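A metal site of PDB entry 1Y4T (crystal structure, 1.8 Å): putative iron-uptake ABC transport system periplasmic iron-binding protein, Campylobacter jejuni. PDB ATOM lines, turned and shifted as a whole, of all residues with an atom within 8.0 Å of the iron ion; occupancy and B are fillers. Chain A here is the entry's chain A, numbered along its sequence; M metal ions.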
ATOM      1  N   ALA A   9     -26.112  18.133 -17.720  1.00  0.00           N
ATOM      2  CA  ALA A   9     -26.759  19.368 -17.311  1.00  0.00           C
ATOM      3  C   ALA A   9     -25.745  20.490 -17.071  1.00  0.00           C
ATOM      4  O   ALA A   9     -26.130  21.603 -16.782  1.00  0.00           O
ATOM      5  CB  ALA A   9     -27.596  19.149 -16.069  1.00  0.00           C
ATOM      6  N   ARG A  10     -24.462  20.201 -17.215  1.00  0.00           N
ATOM      7  CA  ARG A  10     -23.465  21.274 -17.253  1.00  0.00           C
ATOM      8  C   ARG A  10     -23.687  22.159 -18.478  1.00  0.00           C
ATOM      9  O   ARG A  10     -24.373  21.772 -19.430  1.00  0.00           O
ATOM     10  CB  ARG A  10     -22.027  20.732 -17.194  1.00  0.00           C
ATOM     11  CG  ARG A  10     -21.667  20.177 -15.823  1.00  0.00           C
ATOM     12  CD  ARG A  10     -20.294  19.524 -15.769  1.00  0.00           C
ATOM     13  NE  ARG A  10     -19.209  20.433 -16.150  1.00  0.00           N
ATOM     14  CZ  ARG A  10     -18.507  21.219 -15.323  1.00  0.00           C
ATOM     15  NH1 ARG A  10     -18.732  21.198 -14.030  1.00  0.00           N
ATOM     16  NH2 ARG A  10     -17.525  21.973 -15.809  1.00  0.00           N
ATOM     17  N   HIS A  11     -23.130  23.360 -18.438  1.00  0.00           N
ATOM     18  CA  HIS A  11     -23.468  24.347 -19.452  1.00  0.00           C
ATOM     19  C   HIS A  11     -22.284  25.288 -19.695  1.00  0.00           C
ATOM     20  O   HIS A  11     -22.433  26.519 -19.683  1.00  0.00           O
ATOM     21  CB  HIS A  11     -24.704  25.123 -19.001  1.00  0.00           C
ATOM     22  CG  HIS A  11     -24.714  25.474 -17.543  1.00  0.00           C
ATOM     23  ND1 HIS A  11     -25.124  24.573 -16.579  1.00  0.00           N
ATOM     24  CD2 HIS A  11     -24.386  26.603 -16.895  1.00  0.00           C
ATOM     25  CE1 HIS A  11     -25.021  25.146 -15.394  1.00  0.00           C
ATOM     26  NE2 HIS A  11     -24.579  26.384 -15.554  1.00  0.00           N
ATOM     27  N   TYR A  12     -21.118  24.691 -19.945  1.00  0.00           N
ATOM     28  CA  TYR A  12     -19.839  25.400 -19.973  1.00  0.00           C
ATOM     29  C   TYR A  12     -19.013  25.051 -21.210  1.00  0.00           C
ATOM     30  O   TYR A  12     -18.779  23.877 -21.495  1.00  0.00           O
ATOM     31  CB  TYR A  12     -19.032  25.033 -18.738  1.00  0.00           C
ATOM     32  CG  TYR A  12     -19.828  25.122 -17.439  1.00  0.00           C
ATOM     33  CD1 TYR A  12     -20.131  23.986 -16.681  1.00  0.00           C
ATOM     34  CD2 TYR A  12     -20.276  26.344 -16.964  1.00  0.00           C
ATOM     35  CE1 TYR A  12     -20.873  24.075 -15.502  1.00  0.00           C
ATOM     36  CE2 TYR A  12     -21.016  26.443 -15.770  1.00  0.00           C
ATOM     37  CZ  TYR A  12     -21.300  25.301 -15.060  1.00  0.00           C
ATOM     38  OH  TYR A  12     -22.018  25.414 -13.922  1.00  0.00           O
ATOM     39  N   ALA A  59     -24.708  19.743 -12.472  1.00  0.00           N
ATOM     40  CA  ALA A  59     -24.091  20.872 -11.770  1.00  0.00           C
ATOM     41  C   ALA A  59     -24.750  21.010 -10.414  1.00  0.00           C
ATOM     42  O   ALA A  59     -24.843  22.110  -9.869  1.00  0.00           O
ATOM     43  CB  ALA A  59     -24.244  22.124 -12.568  1.00  0.00           C
ATOM     44  N   ASP A  60     -25.226  19.903  -9.858  1.00  0.00           N
ATOM     45  CA  ASP A  60     -25.936  19.975  -8.577  1.00  0.00           C
ATOM     46  C   ASP A  60     -26.067  18.623  -7.911  1.00  0.00           C
ATOM     47  O   ASP A  60     -26.278  17.592  -8.594  1.00  0.00           O
ATOM     48  CB  ASP A  60     -27.333  20.577  -8.841  1.00  0.00           C
ATOM     49  CG  ASP A  60     -28.270  20.465  -7.652  1.00  0.00           C
ATOM     50  OD1 ASP A  60     -29.284  19.766  -7.776  1.00  0.00           O
ATOM     51  OD2 ASP A  60     -28.077  21.043  -6.589  1.00  0.00           O
ATOM     52  N   ARG A 102     -18.394  24.167  -5.794  1.00  0.00           N
ATOM     53  CA  ARG A 102     -18.727  25.547  -6.027  1.00  0.00           C
ATOM     54  C   ARG A 102     -19.449  26.103  -4.808  1.00  0.00           C
ATOM     55  O   ARG A 102     -20.076  25.366  -4.060  1.00  0.00           O
ATOM     56  CB  ARG A 102     -19.556  25.690  -7.311  1.00  0.00           C
ATOM     57  CG  ARG A 102     -20.782  24.788  -7.400  1.00  0.00           C
ATOM     58  CD  ARG A 102     -20.619  23.520  -8.239  1.00  0.00           C
ATOM     59  NE  ARG A 102     -20.276  23.741  -9.627  1.00  0.00           N
ATOM     60  CZ  ARG A 102     -21.127  24.138 -10.578  1.00  0.00           C
ATOM     61  NH1 ARG A 102     -22.403  24.406 -10.313  1.00  0.00           N
ATOM     62  NH2 ARG A 102     -20.665  24.314 -11.824  1.00  0.00           N
ATOM     63  N   ARG A 104     -22.211  28.939  -3.337  1.00  0.00           N
ATOM     64  CA  ARG A 104     -23.235  29.928  -3.645  1.00  0.00           C
ATOM     65  C   ARG A 104     -23.135  31.080  -2.651  1.00  0.00           C
ATOM     66  O   ARG A 104     -23.426  30.940  -1.472  1.00  0.00           O
ATOM     67  CB  ARG A 104     -24.636  29.303  -3.650  1.00  0.00           C
ATOM     68  CG  ARG A 104     -25.657  30.078  -4.454  1.00  0.00           C
ATOM     69  CD  ARG A 104     -26.777  29.228  -4.994  1.00  0.00           C
ATOM     70  NE  ARG A 104     -27.627  29.968  -5.907  1.00  0.00           N
ATOM     71  CZ  ARG A 104     -27.284  30.309  -7.152  1.00  0.00           C
ATOM     72  NH1 ARG A 104     -26.104  29.959  -7.641  1.00  0.00           N
ATOM     73  NH2 ARG A 104     -28.134  30.955  -7.897  1.00  0.00           N
ATOM     74  N   ARG A 137     -32.151  34.107  -9.235  1.00  0.00           N
ATOM     75  CA  ARG A 137     -32.803  33.393 -10.319  1.00  0.00           C
ATOM     76  C   ARG A 137     -33.996  32.588  -9.794  1.00  0.00           C
ATOM     77  O   ARG A 137     -34.217  32.468  -8.580  1.00  0.00           O
ATOM     78  CB  ARG A 137     -31.825  32.473 -11.045  1.00  0.00           C
ATOM     79  CG  ARG A 137     -31.390  31.250 -10.243  1.00  0.00           C
ATOM     80  CD  ARG A 137     -30.245  30.525 -10.877  1.00  0.00           C
ATOM     81  NE  ARG A 137     -30.566  30.033 -12.203  1.00  0.00           N
ATOM     82  CZ  ARG A 137     -29.672  29.558 -13.077  1.00  0.00           C
ATOM     83  NH1 ARG A 137     -28.370  29.579 -12.795  1.00  0.00           N
ATOM     84  NH2 ARG A 137     -30.065  29.115 -14.265  1.00  0.00           N
ATOM     85  N   TYR A 143     -29.673  25.247  -8.490  1.00  0.00           N
ATOM     86  CA  TYR A 143     -28.935  26.005  -7.454  1.00  0.00           C
ATOM     87  C   TYR A 143     -29.870  26.583  -6.393  1.00  0.00           C
ATOM     88  O   TYR A 143     -29.529  26.604  -5.223  1.00  0.00           O
ATOM     89  CB  TYR A 143     -28.086  27.145  -8.019  1.00  0.00           C
ATOM     90  CG  TYR A 143     -27.222  26.771  -9.199  1.00  0.00           C
ATOM     91  CD1 TYR A 143     -26.754  25.466  -9.373  1.00  0.00           C
ATOM     92  CD2 TYR A 143     -26.910  27.709 -10.186  1.00  0.00           C
ATOM     93  CE1 TYR A 143     -25.980  25.119 -10.476  1.00  0.00           C
ATOM     94  CE2 TYR A 143     -26.142  27.370 -11.281  1.00  0.00           C
ATOM     95  CZ  TYR A 143     -25.672  26.075 -11.404  1.00  0.00           C
ATOM     96  OH  TYR A 143     -24.940  25.732 -12.498  1.00  0.00           O
ATOM     97  N   ASP A 179     -27.361  33.072 -13.129  1.00  0.00           N
ATOM     98  CA  ASP A 179     -26.450  33.776 -12.238  1.00  0.00           C
ATOM     99  C   ASP A 179     -25.766  34.954 -12.869  1.00  0.00           C
ATOM    100  O   ASP A 179     -25.625  35.996 -12.265  1.00  0.00           O
ATOM    101  CB  ASP A 179     -25.360  32.824 -11.742  1.00  0.00           C
ATOM    102  CG  ASP A 179     -25.871  31.826 -10.732  1.00  0.00           C
ATOM    103  OD1 ASP A 179     -27.064  31.464 -10.779  1.00  0.00           O
ATOM    104  OD2 ASP A 179     -25.152  31.331  -9.853  1.00  0.00           O
ATOM    105  N   ARG A 180     -25.312  34.795 -14.108  1.00  0.00           N
ATOM    106  CA  ARG A 180     -24.602  35.906 -14.765  1.00  0.00           C
ATOM    107  C   ARG A 180     -25.547  37.088 -15.014  1.00  0.00           C
ATOM    108  O   ARG A 180     -25.111  38.211 -15.011  1.00  0.00           O
ATOM    109  CB  ARG A 180     -23.952  35.443 -16.078  1.00  0.00           C
ATOM    110  CG  ARG A 180     -22.696  34.600 -15.880  1.00  0.00           C
ATOM    111  CD  ARG A 180     -22.135  34.042 -17.165  1.00  0.00           C
ATOM    112  NE  ARG A 180     -22.816  32.828 -17.547  1.00  0.00           N
ATOM    113  CZ  ARG A 180     -22.278  31.814 -18.240  1.00  0.00           C
ATOM    114  NH1 ARG A 180     -21.017  31.840 -18.673  1.00  0.00           N
ATOM    115  NH2 ARG A 180     -23.036  30.760 -18.500  1.00  0.00           N
ATOM    116  N   ASN A 197     -23.172  31.646  -7.884  1.00  0.00           N
ATOM    117  CA  ASN A 197     -22.020  30.748  -7.699  1.00  0.00           C
ATOM    118  C   ASN A 197     -20.678  31.419  -7.965  1.00  0.00           C
ATOM    119  O   ASN A 197     -20.548  32.268  -8.840  1.00  0.00           O
ATOM    120  CB  ASN A 197     -22.153  29.499  -8.605  1.00  0.00           C
ATOM    121  CG  ASN A 197     -23.245  28.548  -8.151  1.00  0.00           C
ATOM    122  OD1 ASN A 197     -23.661  28.592  -6.983  1.00  0.00           O
ATOM    123  ND2 ASN A 197     -23.694  27.668  -9.052  1.00  0.00           N
ATOM    124  N   TYR A 199     -17.896  30.556  -9.430  1.00  0.00           N
ATOM    125  CA  TYR A 199     -17.147  30.348 -10.688  1.00  0.00           C
ATOM    126  C   TYR A 199     -17.601  31.339 -11.764  1.00  0.00           C
ATOM    127  O   TYR A 199     -16.802  31.709 -12.609  1.00  0.00           O
ATOM    128  CB  TYR A 199     -17.210  28.871 -11.193  1.00  0.00           C
ATOM    129  CG  TYR A 199     -18.624  28.378 -11.371  1.00  0.00           C
ATOM    130  CD1 TYR A 199     -19.340  28.606 -12.551  1.00  0.00           C
ATOM    131  CD2 TYR A 199     -19.281  27.723 -10.335  1.00  0.00           C
ATOM    132  CE1 TYR A 199     -20.661  28.166 -12.699  1.00  0.00           C
ATOM    133  CE2 TYR A 199     -20.585  27.306 -10.458  1.00  0.00           C
ATOM    134  CZ  TYR A 199     -21.271  27.538 -11.630  1.00  0.00           C
ATOM    135  OH  TYR A 199     -22.563  27.101 -11.712  1.00  0.00           O
ATOM    136  N   TYR A 200     -18.862  31.814 -11.694  1.00  0.00           N
ATOM    137  CA  TYR A 200     -19.394  32.793 -12.666  1.00  0.00           C
ATOM    138  C   TYR A 200     -18.591  34.079 -12.615  1.00  0.00           C
ATOM    139  O   TYR A 200     -18.398  34.728 -13.637  1.00  0.00           O
ATOM    140  CB  TYR A 200     -20.896  33.050 -12.475  1.00  0.00           C
ATOM    141  CG  TYR A 200     -21.760  31.861 -12.876  1.00  0.00           C
ATOM    142  CD1 TYR A 200     -21.793  31.411 -14.193  1.00  0.00           C
ATOM    143  CD2 TYR A 200     -22.509  31.154 -11.927  1.00  0.00           C
ATOM    144  CE1 TYR A 200     -22.576  30.304 -14.569  1.00  0.00           C
ATOM    145  CE2 TYR A 200     -23.271  30.039 -12.279  1.00  0.00           C
ATOM    146  CZ  TYR A 200     -23.308  29.619 -13.596  1.00  0.00           C
ATOM    147  OH  TYR A 200     -24.059  28.506 -13.965  1.00  0.00           O
ATOM    148  N   LEU A 203     -15.674  33.336 -14.718  1.00  0.00           N
ATOM    149  CA  LEU A 203     -16.085  33.247 -16.118  1.00  0.00           C
ATOM    150  C   LEU A 203     -16.315  34.647 -16.699  1.00  0.00           C
ATOM    151  O   LEU A 203     -15.878  34.948 -17.841  1.00  0.00           O
ATOM    152  CB  LEU A 203     -17.347  32.371 -16.286  1.00  0.00           C
ATOM    153  CG  LEU A 203     -17.177  30.858 -16.125  1.00  0.00           C
ATOM    154  CD1 LEU A 203     -18.524  30.140 -16.176  1.00  0.00           C
ATOM    155  CD2 LEU A 203     -16.285  30.334 -17.207  1.00  0.00           C
ATOM    156  N   SER A 236     -20.669  19.904  -8.784  1.00  0.00           N
ATOM    157  CA  SER A 236     -20.963  19.325 -10.078  1.00  0.00           C
ATOM    158  C   SER A 236     -20.542  17.877  -9.892  1.00  0.00           C
ATOM    159  O   SER A 236     -19.521  17.610  -9.248  1.00  0.00           O
ATOM    160  CB  SER A 236     -20.123  20.007 -11.161  1.00  0.00           C
ATOM    161  OG  SER A 236     -20.353  19.437 -12.426  1.00  0.00           O
ATOM    162  N   ASN A 270     -12.694  26.871 -16.018  1.00  0.00           N
ATOM    163  CA  ASN A 270     -14.079  27.081 -15.591  1.00  0.00           C
ATOM    164  C   ASN A 270     -14.233  27.705 -14.207  1.00  0.00           C
ATOM    165  O   ASN A 270     -15.343  27.954 -13.768  1.00  0.00           O
ATOM    166  CB  ASN A 270     -14.933  25.809 -15.732  1.00  0.00           C
ATOM    167  CG  ASN A 270     -16.380  26.122 -16.118  1.00  0.00           C
ATOM    168  OD1 ASN A 270     -16.626  26.829 -17.104  1.00  0.00           O
ATOM    169  ND2 ASN A 270     -17.335  25.580 -15.367  1.00  0.00           N
ATOM    170  N   GLU A 272     -13.860  26.654 -11.239  1.00  0.00           N
ATOM    171  CA  GLU A 272     -14.505  25.859 -10.174  1.00  0.00           C
ATOM    172  C   GLU A 272     -13.435  25.432  -9.183  1.00  0.00           C
ATOM    173  O   GLU A 272     -12.262  25.604  -9.455  1.00  0.00           O
ATOM    174  CB  GLU A 272     -15.238  24.652 -10.755  1.00  0.00           C
ATOM    175  CG  GLU A 272     -16.464  25.023 -11.567  1.00  0.00           C
ATOM    176  CD  GLU A 272     -17.042  23.830 -12.297  1.00  0.00           C
ATOM    177  OE1 GLU A 272     -16.574  23.509 -13.414  1.00  0.00           O
ATOM    178  OE2 GLU A 272     -17.963  23.225 -11.733  1.00  0.00           O
HETATM  179 FE    FE M   1     -23.498  26.712 -13.572  1.00  0.00          FE
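The nearest printed residue that does not touch the iron ion is Arg 102 (4.1 Å).
The iron ion is bound by OH of Tyr 200, 1.9 Å away.
The iron ion is bound by the side-chain hydroxyl (OH) of Tyr 12 (2.0 Å).
The iron ion is bound by OH of Tyr 143 (2.0 Å).
The side-chain hydroxyl (OH) of Tyr 199 binds the iron ion (2.1 Å).
NE2 of His 11 binds the iron ion (2.3 Å).
The iron ion has five donor atoms within binding distance.
The guanidinium group (NH2) of Arg 102 sits close to the side-chain hydroxyl (OH) of Tyr 12, at 2.7 Å.
The side-chain hydroxyl (OH) of Tyr 199 sits close to the guanidinium group (NH1) of Arg 102, at 3.0 Å.
ND1 of His 11 sits at hydrogen-bond distance from O of Ala 9, 3.1 Å away.
The side-chain hydroxyl (OH) of Tyr 199 lies close to the side-chain amide nitrogen (ND2) of Asn 197 (2.9 Å).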
